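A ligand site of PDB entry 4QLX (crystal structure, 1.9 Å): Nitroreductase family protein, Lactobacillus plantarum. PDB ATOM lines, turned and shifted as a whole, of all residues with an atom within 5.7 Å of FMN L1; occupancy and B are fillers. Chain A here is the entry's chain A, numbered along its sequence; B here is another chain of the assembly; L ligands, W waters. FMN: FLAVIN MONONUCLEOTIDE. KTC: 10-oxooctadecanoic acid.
The side-chain hydroxyl (OG) of Ser 24 is in hydrogen-bond range of the side-chain amide nitrogen (ND2) of Asn 167 (3.2 Å).
The side-chain amide nitrogen of Gln 83 lies within hydrogen-bond range of the side-chain amide oxygen of Asn 167 (3.0 Å).
O of Arg 26 sits close to N of Gln 83 (3.4 Å).
The guanidinium group of Arg 22 lies within hydrogen-bond range of the backbone carbonyl oxygen of Thr 48 of chain B (2.9 Å).
The side-chain amide nitrogen (NE2) of Gln 83 is in hydrogen-bond range of the side-chain amide oxygen (OD1) of Asn 80, 3.0 Å away.
The backbone NH (N) of Ala 52 of chain B is in hydrogen-bond range of the side-chain carboxylate (OD1) of Asp 147 of chain B (3.1 Å).
The side-chain amide nitrogen (ND2) of Asn 80 lies within hydrogen-bond range of the backbone carbonyl oxygen (O) of Gly 171, 3.1 Å away.
The backbone carbonyl oxygen (O) of Cys 53 of chain B is in hydrogen-bond range of the indole nitrogen (NE1) of Trp 107 of chain B (2.9 Å).
An oxygen (O2') of FMN L1 sits at hydrogen-bond distance from an oxygen (O2) of KTC L2.
The backbone NH of Ser 24 sits at hydrogen-bond distance from an oxygen (O1P) of FMN L1, at 2.7 Å.
The backbone NH (N) of Cys 53 of chain B sits at hydrogen-bond distance from an oxygen (O2) of KTC L2, 2.7 Å away.
The guanidinium group (NH1) of Arg 22 lies within salt-bridge range of an oxygen (O2P) of FMN L1, at 2.8 Å.
N of Gly 171 sits at hydrogen-bond distance from O4 of FMN L1, 3.1 Å away.
A nitrogen (N3) of FMN L1 sits at hydrogen-bond distance from the side-chain amide oxygen (OD1) of Asn 80 (2.7 Å).
N of Ser 170 sits at hydrogen-bond distance from N5 of FMN L1 (3.1 Å).
An oxygen (O2) of FMN L1 sits at hydrogen-bond distance from the guanidinium group (NE) of Arg 26 (2.7 Å).
An oxygen (O2P) of FMN L1 is in hydrogen-bond range of the side-chain hydroxyl of Ser 24 (2.8 Å).
ND2 of Asn 167 lies close to N1 of FMN L1, 3.5 Å away.
The side-chain amide nitrogen (NE2) of Gln 83 lies within hydrogen-bond range of an oxygen (O2) of FMN L1, at 3.2 Å.
Water W1 lies within hydrogen-bond range of an oxygen (O3P) of FMN L1 (2.5 Å), the backbone carbonyl oxygen (O) of Arg 22 (2.9 Å) and a ring nitrogen (ND1) of His 23 (3.3 Å).
Water W4 bridges O1P of FMN L1 and ND1 of His 23.
Water W2 lies within hydrogen-bond range of the guanidinium group (NH2) of Arg 26 and an oxygen (O5') of FMN L1.
Water W3 lies within hydrogen-bond range of O of Asp 143 of chain B (2.5 Å) and OD1 of Asp 147 of chain B (2.6 Å).
Water W5 lies within hydrogen-bond range of O of Ser 24 (2.9 Å), NH1 of Arg 26 (3.0 Å) and O1P of FMN L1 (3.3 Å).
A nitrogen (N10) of FMN L1 sits close to the backbone carbonyl oxygen (O) of Ala 168 (2.9 Å).
Merely in contact with FMN L1: Pro 50 of chain B, Phe 169, Ser 51 of chain B, Asn 54 of chain B, Ala 52 of chain B, His 23, Ile 146 of chain B, Phe 79, Cys 53 of chain B and Asp 147 of chain B.
Hydrophobic or aromatic side chains within 4 Å of FMN L1: His 23, Phe 79, Phe 169, Pro 50 of chain B, Ala 52 of chain B and Ile 146 of chain B.
19 residues have an atom within 4 Å of FMN L1: Arg 22, His 23, Ser 24, Arg 26, Phe 79, Asn 80, Gln 83, Asn 167, Ala 168, Phe 169, Ser 170, Gly 171, Pro 50 of chain B, Ser 51 of chain B, Ala 52 of chain B, Cys 53 of chain B, Asn 54 of chain B, Ile 146 of chain B and Asp 147 of chain B.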
ATOM      1  N   ARG A  22     -10.805  -7.918   6.210  1.00  0.00           N
ATOM      2  CA  ARG A  22     -10.191  -9.232   6.120  1.00  0.00           C
ATOM      3  C   ARG A  22     -11.259 -10.274   5.783  1.00  0.00           C
ATOM      4  O   ARG A  22     -12.309 -10.320   6.407  1.00  0.00           O
ATOM      5  CB  ARG A  22      -9.502  -9.620   7.444  1.00  0.00           C
ATOM      6  CG  ARG A  22      -8.807 -10.979   7.372  1.00  0.00           C
ATOM      7  CD  ARG A  22      -8.732 -11.680   8.713  1.00  0.00           C
ATOM      8  NE  ARG A  22     -10.050 -11.771   9.336  1.00  0.00           N
ATOM      9  CZ  ARG A  22     -10.970 -12.676   9.021  1.00  0.00           C
ATOM     10  NH1 ARG A  22     -10.726 -13.595   8.076  1.00  0.00           N
ATOM     11  NH2 ARG A  22     -12.144 -12.656   9.642  1.00  0.00           N
ATOM     12  N   HIS A  23     -10.973 -11.122   4.800  1.00  0.00           N
ATOM     13  CA  HIS A  23     -11.829 -12.256   4.522  1.00  0.00           C
ATOM     14  C   HIS A  23     -10.987 -13.494   4.335  1.00  0.00           C
ATOM     15  O   HIS A  23      -9.842 -13.398   3.905  1.00  0.00           O
ATOM     16  CB  HIS A  23     -12.693 -12.008   3.265  1.00  0.00           C
ATOM     17  CG  HIS A  23     -13.560 -10.788   3.352  1.00  0.00           C
ATOM     18  ND1 HIS A  23     -14.807 -10.814   3.935  1.00  0.00           N
ATOM     19  CD2 HIS A  23     -13.368  -9.526   2.932  1.00  0.00           C
ATOM     20  CE1 HIS A  23     -15.346  -9.610   3.878  1.00  0.00           C
ATOM     21  NE2 HIS A  23     -14.492  -8.805   3.265  1.00  0.00           N
ATOM     22  N   SER A  24     -11.561 -14.652   4.631  1.00  0.00           N
ATOM     23  CA  SER A  24     -10.943 -15.902   4.273  1.00  0.00           C
ATOM     24  C   SER A  24     -10.859 -16.033   2.765  1.00  0.00           C
ATOM     25  O   SER A  24     -11.878 -16.073   2.076  1.00  0.00           O
ATOM     26  CB  SER A  24     -11.715 -17.078   4.856  1.00  0.00           C
ATOM     27  OG  SER A  24     -11.339 -17.281   6.204  1.00  0.00           O
ATOM     28  N   ARG A  26      -9.501 -18.545  -0.249  1.00  0.00           N
ATOM     29  CA  ARG A  26      -9.206 -19.961  -0.374  1.00  0.00           C
ATOM     30  C   ARG A  26      -8.616 -20.320  -1.746  1.00  0.00           C
ATOM     31  O   ARG A  26      -8.024 -21.381  -1.906  1.00  0.00           O
ATOM     32  CB  ARG A  26     -10.482 -20.785  -0.119  1.00  0.00           C
ATOM     33  CG  ARG A  26     -10.920 -20.787   1.337  1.00  0.00           C
ATOM     34  CD  ARG A  26     -12.304 -21.386   1.534  1.00  0.00           C
ATOM     35  NE  ARG A  26     -12.737 -21.247   2.923  1.00  0.00           N
ATOM     36  CZ  ARG A  26     -13.401 -20.198   3.393  1.00  0.00           C
ATOM     37  NH1 ARG A  26     -13.726 -19.189   2.587  1.00  0.00           N
ATOM     38  NH2 ARG A  26     -13.740 -20.146   4.677  1.00  0.00           N
ATOM     39  N   PHE A  79     -11.547 -31.311   1.561  1.00  0.00           N
ATOM     40  CA  PHE A  79     -12.260 -30.038   1.492  1.00  0.00           C
ATOM     41  C   PHE A  79     -11.283 -28.852   1.393  1.00  0.00           C
ATOM     42  O   PHE A  79     -11.585 -27.848   0.757  1.00  0.00           O
ATOM     43  CB  PHE A  79     -13.169 -29.876   2.720  1.00  0.00           C
ATOM     44  CG  PHE A  79     -14.060 -28.651   2.674  1.00  0.00           C
ATOM     45  CD1 PHE A  79     -13.602 -27.415   3.091  1.00  0.00           C
ATOM     46  CD2 PHE A  79     -15.371 -28.767   2.215  1.00  0.00           C
ATOM     47  CE1 PHE A  79     -14.436 -26.296   3.040  1.00  0.00           C
ATOM     48  CE2 PHE A  79     -16.202 -27.658   2.178  1.00  0.00           C
ATOM     49  CZ  PHE A  79     -15.732 -26.426   2.590  1.00  0.00           C
ATOM     50  N   ASN A  80     -10.104 -28.987   1.995  1.00  0.00           N
ATOM     51  CA  ASN A  80      -9.146 -27.891   2.037  1.00  0.00           C
ATOM     52  C   ASN A  80      -8.020 -27.986   1.012  1.00  0.00           C
ATOM     53  O   ASN A  80      -7.076 -27.215   1.061  1.00  0.00           O
ATOM     54  CB  ASN A  80      -8.563 -27.792   3.445  1.00  0.00           C
ATOM     55  CG  ASN A  80      -9.585 -27.318   4.439  1.00  0.00           C
ATOM     56  OD1 ASN A  80     -10.335 -26.389   4.157  1.00  0.00           O
ATOM     57  ND2 ASN A  80      -9.649 -27.969   5.586  1.00  0.00           N
ATOM     58  N   GLN A  83      -7.085 -24.496  -1.065  1.00  0.00           N
ATOM     59  CA  GLN A  83      -6.159 -23.623  -0.356  1.00  0.00           C
ATOM     60  C   GLN A  83      -4.735 -24.154  -0.433  1.00  0.00           C
ATOM     61  O   GLN A  83      -3.819 -23.422  -0.789  1.00  0.00           O
ATOM     62  CB  GLN A  83      -6.568 -23.479   1.103  1.00  0.00           C
ATOM     63  CG  GLN A  83      -7.953 -22.920   1.305  1.00  0.00           C
ATOM     64  CD  GLN A  83      -8.982 -23.979   1.629  1.00  0.00           C
ATOM     65  OE1 GLN A  83      -9.249 -24.876   0.832  1.00  0.00           O
ATOM     66  NE2 GLN A  83      -9.571 -23.870   2.815  1.00  0.00           N
ATOM     67  N   ASN A 167      -6.137 -17.801   4.586  1.00  0.00           N
ATOM     68  CA  ASN A 167      -7.189 -18.573   5.202  1.00  0.00           C
ATOM     69  C   ASN A 167      -6.612 -19.384   6.335  1.00  0.00           C
ATOM     70  O   ASN A 167      -5.587 -20.055   6.161  1.00  0.00           O
ATOM     71  CB  ASN A 167      -7.872 -19.494   4.179  1.00  0.00           C
ATOM     72  CG  ASN A 167      -8.790 -20.523   4.827  1.00  0.00           C
ATOM     73  OD1 ASN A 167      -8.588 -21.726   4.688  1.00  0.00           O
ATOM     74  ND2 ASN A 167      -9.793 -20.046   5.544  1.00  0.00           N
ATOM     75  N   ALA A 168      -7.252 -19.307   7.503  1.00  0.00           N
ATOM     76  CA  ALA A 168      -6.905 -20.177   8.619  1.00  0.00           C
ATOM     77  C   ALA A 168      -7.768 -21.416   8.503  1.00  0.00           C
ATOM     78  O   ALA A 168      -8.921 -21.331   8.075  1.00  0.00           O
ATOM     79  CB  ALA A 168      -7.112 -19.470   9.971  1.00  0.00           C
ATOM     80  N   PHE A 169      -7.201 -22.584   8.821  1.00  0.00           N
ATOM     81  CA  PHE A 169      -7.988 -23.824   8.712  1.00  0.00           C
ATOM     82  C   PHE A 169      -7.498 -24.916   9.648  1.00  0.00           C
ATOM     83  O   PHE A 169      -6.297 -25.108   9.824  1.00  0.00           O
ATOM     84  CB  PHE A 169      -7.984 -24.341   7.259  1.00  0.00           C
ATOM     85  CG  PHE A 169      -6.654 -24.847   6.778  1.00  0.00           C
ATOM     86  CD1 PHE A 169      -5.754 -23.980   6.164  1.00  0.00           C
ATOM     87  CD2 PHE A 169      -6.296 -26.181   6.937  1.00  0.00           C
ATOM     88  CE1 PHE A 169      -4.535 -24.424   5.711  1.00  0.00           C
ATOM     89  CE2 PHE A 169      -5.067 -26.630   6.492  1.00  0.00           C
ATOM     90  CZ  PHE A 169      -4.185 -25.750   5.884  1.00  0.00           C
ATOM     91  N   SER A 170      -8.445 -25.624  10.266  1.00  0.00           N
ATOM     92  CA  SER A 170      -8.121 -26.749  11.127  1.00  0.00           C
ATOM     93  C   SER A 170      -8.820 -28.015  10.664  1.00  0.00           C
ATOM     94  O   SER A 170      -8.889 -28.995  11.417  1.00  0.00           O
ATOM     95  CB  SER A 170      -8.488 -26.440  12.585  1.00  0.00           C
ATOM     96  OG  SER A 170      -9.903 -26.287  12.714  1.00  0.00           O
ATOM     97  N   GLY A 171      -9.306 -28.005   9.426  1.00  0.00           N
ATOM     98  CA  GLY A 171      -9.918 -29.187   8.834  1.00  0.00           C
ATOM     99  C   GLY A 171      -8.823 -30.160   8.454  1.00  0.00           C
ATOM    100  O   GLY A 171      -8.415 -30.226   7.282  1.00  0.00           O
ATOM    101  N   MET A 192      -3.547 -25.333  13.760  1.00  0.00           N
ATOM    102  CA  MET A 192      -4.162 -24.815  12.540  1.00  0.00           C
ATOM    103  C   MET A 192      -3.141 -24.543  11.439  1.00  0.00           C
ATOM    104  O   MET A 192      -1.971 -24.283  11.718  1.00  0.00           O
ATOM    105  CB  MET A 192      -4.958 -23.523  12.825  1.00  0.00           C
ATOM    106  CG  MET A 192      -4.093 -22.322  13.219  1.00  0.00           C
ATOM    107  SD  MET A 192      -4.958 -20.737  13.350  1.00  0.00           S
ATOM    108  CE  MET A 192      -5.730 -20.902  14.972  1.00  0.00           C
ATOM    109  N   THR B  48     -15.057  -9.247  14.411  1.00  0.00           N
ATOM    110  CA  THR B  48     -14.761  -9.411  12.988  1.00  0.00           C
ATOM    111  C   THR B  48     -13.793 -10.563  12.722  1.00  0.00           C
ATOM    112  O   THR B  48     -13.572 -10.965  11.563  1.00  0.00           O
ATOM    113  CB  THR B  48     -14.162  -8.131  12.368  1.00  0.00           C
ATOM    114  OG1 THR B  48     -12.903  -7.842  12.997  1.00  0.00           O
ATOM    115  CG2 THR B  48     -15.108  -6.968  12.545  1.00  0.00           C
ATOM    116  N   ALA B  49     -13.227 -11.115  13.802  1.00  0.00           N
ATOM    117  CA  ALA B  49     -12.300 -12.251  13.746  1.00  0.00           C
ATOM    118  C   ALA B  49     -12.890 -13.469  13.047  1.00  0.00           C
ATOM    119  O   ALA B  49     -14.113 -13.672  13.066  1.00  0.00           O
ATOM    120  CB  ALA B  49     -11.837 -12.643  15.187  1.00  0.00           C
ATOM    121  N   PRO B  50     -12.034 -14.313  12.440  1.00  0.00           N
ATOM    122  CA  PRO B  50     -12.486 -15.618  11.924  1.00  0.00           C
ATOM    123  C   PRO B  50     -12.833 -16.580  13.068  1.00  0.00           C
ATOM    124  O   PRO B  50     -12.420 -16.380  14.209  1.00  0.00           O
ATOM    125  CB  PRO B  50     -11.271 -16.121  11.120  1.00  0.00           C
ATOM    126  CG  PRO B  50     -10.076 -15.482  11.837  1.00  0.00           C
ATOM    127  CD  PRO B  50     -10.595 -14.090  12.231  1.00  0.00           C
ATOM    128  N   SER B  51     -13.592 -17.621  12.750  1.00  0.00           N
ATOM    129  CA  SER B  51     -13.920 -18.658  13.718  1.00  0.00           C
ATOM    130  C   SER B  51     -14.240 -19.881  12.879  1.00  0.00           C
ATOM    131  O   SER B  51     -14.668 -19.739  11.741  1.00  0.00           O
ATOM    132  CB  SER B  51     -15.105 -18.264  14.605  1.00  0.00           C
ATOM    133  OG  SER B  51     -16.278 -18.060  13.829  1.00  0.00           O
ATOM    134  N   ALA B  52     -14.013 -21.073  13.422  1.00  0.00           N
ATOM    135  CA  ALA B  52     -14.229 -22.301  12.659  1.00  0.00           C
ATOM    136  C   ALA B  52     -15.700 -22.431  12.272  1.00  0.00           C
ATOM    137  O   ALA B  52     -16.576 -22.248  13.111  1.00  0.00           O
ATOM    138  CB  ALA B  52     -13.770 -23.521  13.443  1.00  0.00           C
ATOM    139  N   CYS B  53     -15.937 -22.703  10.998  1.00  0.00           N
ATOM    140  CA  CYS B  53     -17.282 -22.786  10.414  1.00  0.00           C
ATOM    141  C   CYS B  53     -18.140 -21.543  10.692  1.00  0.00           C
ATOM    142  O   CYS B  53     -19.358 -21.604  10.644  1.00  0.00           O
ATOM    143  CB  CYS B  53     -17.982 -24.050  10.917  1.00  0.00           C
ATOM    144  SG  CYS B  53     -17.318 -25.585  10.192  1.00  0.00           S
ATOM    145  N   ASN B  54     -17.478 -20.421  10.964  1.00  0.00           N
ATOM    146  CA  ASN B  54     -18.123 -19.153  11.318  1.00  0.00           C
ATOM    147  C   ASN B  54     -19.127 -19.274  12.463  1.00  0.00           C
ATOM    148  O   ASN B  54     -20.086 -18.519  12.533  1.00  0.00           O
ATOM    149  CB  ASN B  54     -18.824 -18.524  10.106  1.00  0.00           C
ATOM    150  CG  ASN B  54     -19.110 -17.043  10.310  1.00  0.00           C
ATOM    151  OD1 ASN B  54     -18.346 -16.363  10.990  1.00  0.00           O
ATOM    152  ND2 ASN B  54     -20.203 -16.551   9.745  1.00  0.00           N
ATOM    153  N   TRP B 107     -25.823 -21.880   7.802  1.00  0.00           N
ATOM    154  CA  TRP B 107     -25.222 -22.102   6.494  1.00  0.00           C
ATOM    155  C   TRP B 107     -26.283 -22.330   5.416  1.00  0.00           C
ATOM    156  O   TRP B 107     -26.050 -22.081   4.238  1.00  0.00           O
ATOM    157  CB  TRP B 107     -24.222 -23.260   6.550  1.00  0.00           C
ATOM    158  CG  TRP B 107     -22.907 -22.822   7.129  1.00  0.00           C
ATOM    159  CD1 TRP B 107     -22.426 -23.093   8.381  1.00  0.00           C
ATOM    160  CD2 TRP B 107     -21.923 -21.987   6.491  1.00  0.00           C
ATOM    161  NE1 TRP B 107     -21.183 -22.498   8.556  1.00  0.00           N
ATOM    162  CE2 TRP B 107     -20.863 -21.810   7.407  1.00  0.00           C
ATOM    163  CE3 TRP B 107     -21.832 -21.382   5.237  1.00  0.00           C
ATOM    164  CZ2 TRP B 107     -19.732 -21.063   7.105  1.00  0.00           C
ATOM    165  CZ3 TRP B 107     -20.708 -20.639   4.941  1.00  0.00           C
ATOM    166  CH2 TRP B 107     -19.669 -20.475   5.874  1.00  0.00           C
ATOM    167  N   PHE B 128     -18.362 -31.046   7.712  1.00  0.00           N
ATOM    168  CA  PHE B 128     -17.997 -30.577   9.046  1.00  0.00           C
ATOM    169  C   PHE B 128     -19.111 -30.732  10.097  1.00  0.00           C
ATOM    170  O   PHE B 128     -18.829 -30.878  11.295  1.00  0.00           O
ATOM    171  CB  PHE B 128     -17.540 -29.121   8.984  1.00  0.00           C
ATOM    172  CG  PHE B 128     -16.364 -28.890   8.088  1.00  0.00           C
ATOM    173  CD1 PHE B 128     -15.087 -29.275   8.485  1.00  0.00           C
ATOM    174  CD2 PHE B 128     -16.527 -28.299   6.838  1.00  0.00           C
ATOM    175  CE1 PHE B 128     -13.993 -29.069   7.644  1.00  0.00           C
ATOM    176  CE2 PHE B 128     -15.446 -28.088   6.002  1.00  0.00           C
ATOM    177  CZ  PHE B 128     -14.176 -28.477   6.406  1.00  0.00           C
ATOM    178  N   ASP B 143     -12.011 -26.529  20.071  1.00  0.00           N
ATOM    179  CA  ASP B 143     -12.556 -25.696  18.996  1.00  0.00           C
ATOM    180  C   ASP B 143     -12.940 -24.290  19.465  1.00  0.00           C
ATOM    181  O   ASP B 143     -12.579 -23.294  18.831  1.00  0.00           O
ATOM    182  CB  ASP B 143     -13.789 -26.378  18.377  1.00  0.00           C
ATOM    183  CG  ASP B 143     -14.440 -25.552  17.268  1.00  0.00           C
ATOM    184  OD1 ASP B 143     -14.112 -25.760  16.085  1.00  0.00           O
ATOM    185  OD2 ASP B 143     -15.309 -24.702  17.578  1.00  0.00           O
ATOM    186  N   ILE B 146      -9.940 -22.024  20.489  1.00  0.00           N
ATOM    187  CA  ILE B 146      -9.280 -21.399  19.352  1.00  0.00           C
ATOM    188  C   ILE B 146     -10.006 -20.131  18.906  1.00  0.00           C
ATOM    189  O   ILE B 146      -9.382 -19.079  18.791  1.00  0.00           O
ATOM    190  CB  ILE B 146      -9.169 -22.358  18.171  1.00  0.00           C
ATOM    191  CG1 ILE B 146      -8.191 -23.487  18.507  1.00  0.00           C
ATOM    192  CG2 ILE B 146      -8.686 -21.608  16.955  1.00  0.00           C
ATOM    193  CD1 ILE B 146      -7.981 -24.491  17.384  1.00  0.00           C
ATOM    194  N   ASP B 147     -11.318 -20.231  18.672  1.00  0.00           N
ATOM    195  CA  ASP B 147     -12.139 -19.041  18.369  1.00  0.00           C
ATOM    196  C   ASP B 147     -11.951 -17.939  19.413  1.00  0.00           C
ATOM    197  O   ASP B 147     -11.778 -16.757  19.069  1.00  0.00           O
ATOM    198  CB  ASP B 147     -13.637 -19.388  18.320  1.00  0.00           C
ATOM    199  CG  ASP B 147     -14.017 -20.271  17.124  1.00  0.00           C
ATOM    200  OD1 ASP B 147     -13.111 -20.679  16.352  1.00  0.00           O
ATOM    201  OD2 ASP B 147     -15.239 -20.536  16.972  1.00  0.00           O
ATOM    202  N   VAL B 150      -8.584 -16.131  19.082  1.00  0.00           N
ATOM    203  CA  VAL B 150      -8.326 -15.222  17.983  1.00  0.00           C
ATOM    204  C   VAL B 150      -9.109 -13.925  18.199  1.00  0.00           C
ATOM    205  O   VAL B 150      -8.612 -12.838  17.877  1.00  0.00           O
ATOM    206  CB  VAL B 150      -8.638 -15.859  16.608  1.00  0.00           C
ATOM    207  CG1 VAL B 150      -7.689 -17.045  16.365  1.00  0.00           C
ATOM    208  CG2 VAL B 150     -10.099 -16.280  16.481  1.00  0.00           C
HETATM  209  N1  FMN L   1     -12.062 -22.533   6.326  1.00  0.00           N
HETATM  210  C2  FMN L   1     -12.023 -23.621   5.475  1.00  0.00           C
HETATM  211  O2  FMN L   1     -12.336 -23.504   4.305  1.00  0.00           O
HETATM  212  N3  FMN L   1     -11.624 -24.852   5.923  1.00  0.00           N
HETATM  213  C4  FMN L   1     -11.257 -25.002   7.245  1.00  0.00           C
HETATM  214  O4  FMN L   1     -10.907 -26.100   7.659  1.00  0.00           O
HETATM  215  C4A FMN L   1     -11.304 -23.919   8.101  1.00  0.00           C
HETATM  216  N5  FMN L   1     -10.943 -24.085   9.419  1.00  0.00           N
HETATM  217  C5A FMN L   1     -10.952 -23.026  10.288  1.00  0.00           C
HETATM  218  C6  FMN L   1     -10.560 -23.266  11.592  1.00  0.00           C
HETATM  219  C7  FMN L   1     -10.542 -22.224  12.499  1.00  0.00           C
HETATM  220  C7M FMN L   1     -10.116 -22.465  13.917  1.00  0.00           C
HETATM  221  C8  FMN L   1     -10.930 -20.962  12.106  1.00  0.00           C
HETATM  222  C8M FMN L   1     -10.897 -19.873  13.121  1.00  0.00           C
HETATM  223  C9  FMN L   1     -11.329 -20.714  10.780  1.00  0.00           C
HETATM  224  C9A FMN L   1     -11.340 -21.764   9.858  1.00  0.00           C
HETATM  225  N10 FMN L   1     -11.732 -21.594   8.520  1.00  0.00           N
HETATM  226  C10 FMN L   1     -11.695 -22.672   7.655  1.00  0.00           C
HETATM  227  C1' FMN L   1     -12.177 -20.265   7.978  1.00  0.00           C
HETATM  228  C2' FMN L   1     -13.589 -19.935   8.510  1.00  0.00           C
HETATM  229  O2' FMN L   1     -14.568 -20.699   7.850  1.00  0.00           O
HETATM  230  C3' FMN L   1     -13.924 -18.446   8.389  1.00  0.00           C
HETATM  231  O3' FMN L   1     -13.073 -17.731   9.260  1.00  0.00           O
HETATM  232  C4' FMN L   1     -15.364 -18.092   8.759  1.00  0.00           C
HETATM  233  O4' FMN L   1     -16.320 -18.683   7.901  1.00  0.00           O
HETATM  234  C5' FMN L   1     -15.563 -16.575   8.744  1.00  0.00           C
HETATM  235  O5' FMN L   1     -15.255 -16.039   7.466  1.00  0.00           O
HETATM  236  P   FMN L   1     -14.093 -14.930   7.314  1.00  0.00           P
HETATM  237  O1P FMN L   1     -13.992 -14.606   5.845  1.00  0.00           O
HETATM  238  O2P FMN L   1     -12.773 -15.496   7.827  1.00  0.00           O
HETATM  239  O3P FMN L   1     -14.431 -13.686   8.095  1.00  0.00           O
HETATM  240  O1  KTC L   2     -17.281 -21.150  -1.882  1.00  0.00           O
HETATM  241  C17 KTC L   2     -16.791 -20.720  -0.845  1.00  0.00           C
HETATM  242  O   KTC L   2     -16.178 -19.530  -0.836  1.00  0.00           O
HETATM  243  C16 KTC L   2     -16.860 -21.521   0.433  1.00  0.00           C
HETATM  244  C15 KTC L   2     -17.565 -20.691   1.490  1.00  0.00           C
HETATM  245  C14 KTC L   2     -16.927 -20.898   2.848  1.00  0.00           C
HETATM  246  C13 KTC L   2     -17.091 -22.340   3.330  1.00  0.00           C
HETATM  247  C12 KTC L   2     -16.546 -22.510   4.739  1.00  0.00           C
HETATM  248  C11 KTC L   2     -17.078 -23.797   5.349  1.00  0.00           C
HETATM  249  C10 KTC L   2     -16.550 -23.999   6.766  1.00  0.00           C
HETATM  250  C9  KTC L   2     -15.074 -24.392   6.752  1.00  0.00           C
HETATM  251  C8  KTC L   2     -14.579 -24.345   8.169  1.00  0.00           C
HETATM  252  O2  KTC L   2     -14.526 -23.279   8.783  1.00  0.00           O
HETATM  253  C7  KTC L   2     -14.145 -25.631   8.835  1.00  0.00           C
HETATM  254  C6  KTC L   2     -13.702 -25.323  10.257  1.00  0.00           C
HETATM  255  C5  KTC L   2     -12.699 -26.363  10.727  1.00  0.00           C
HETATM  256  C4  KTC L   2     -13.404 -27.459  11.508  1.00  0.00           C
HETATM  257  C3  KTC L   2     -12.579 -28.727  11.402  1.00  0.00           C
HETATM  258  C2  KTC L   2     -12.515 -29.447  12.732  1.00  0.00           C
HETATM  259  C1  KTC L   2     -12.335 -30.958  12.514  1.00  0.00           C
HETATM  260  C   KTC L   2     -11.172 -31.296  11.606  1.00  0.00           C
HETATM  261  O   HOH W   1     -14.905 -11.415   7.184  1.00  0.00           O
HETATM  262  O   HOH W   2     -15.401 -17.950   4.996  1.00  0.00           O
HETATM  263  O   HOH W   3     -12.159 -23.049  16.389  1.00  0.00           O
HETATM  264  O   HOH W   4     -15.774 -13.262   4.641  1.00  0.00           O
HETATM  265  O   HOH W   5     -14.552 -16.309   3.038  1.00  0.00           O
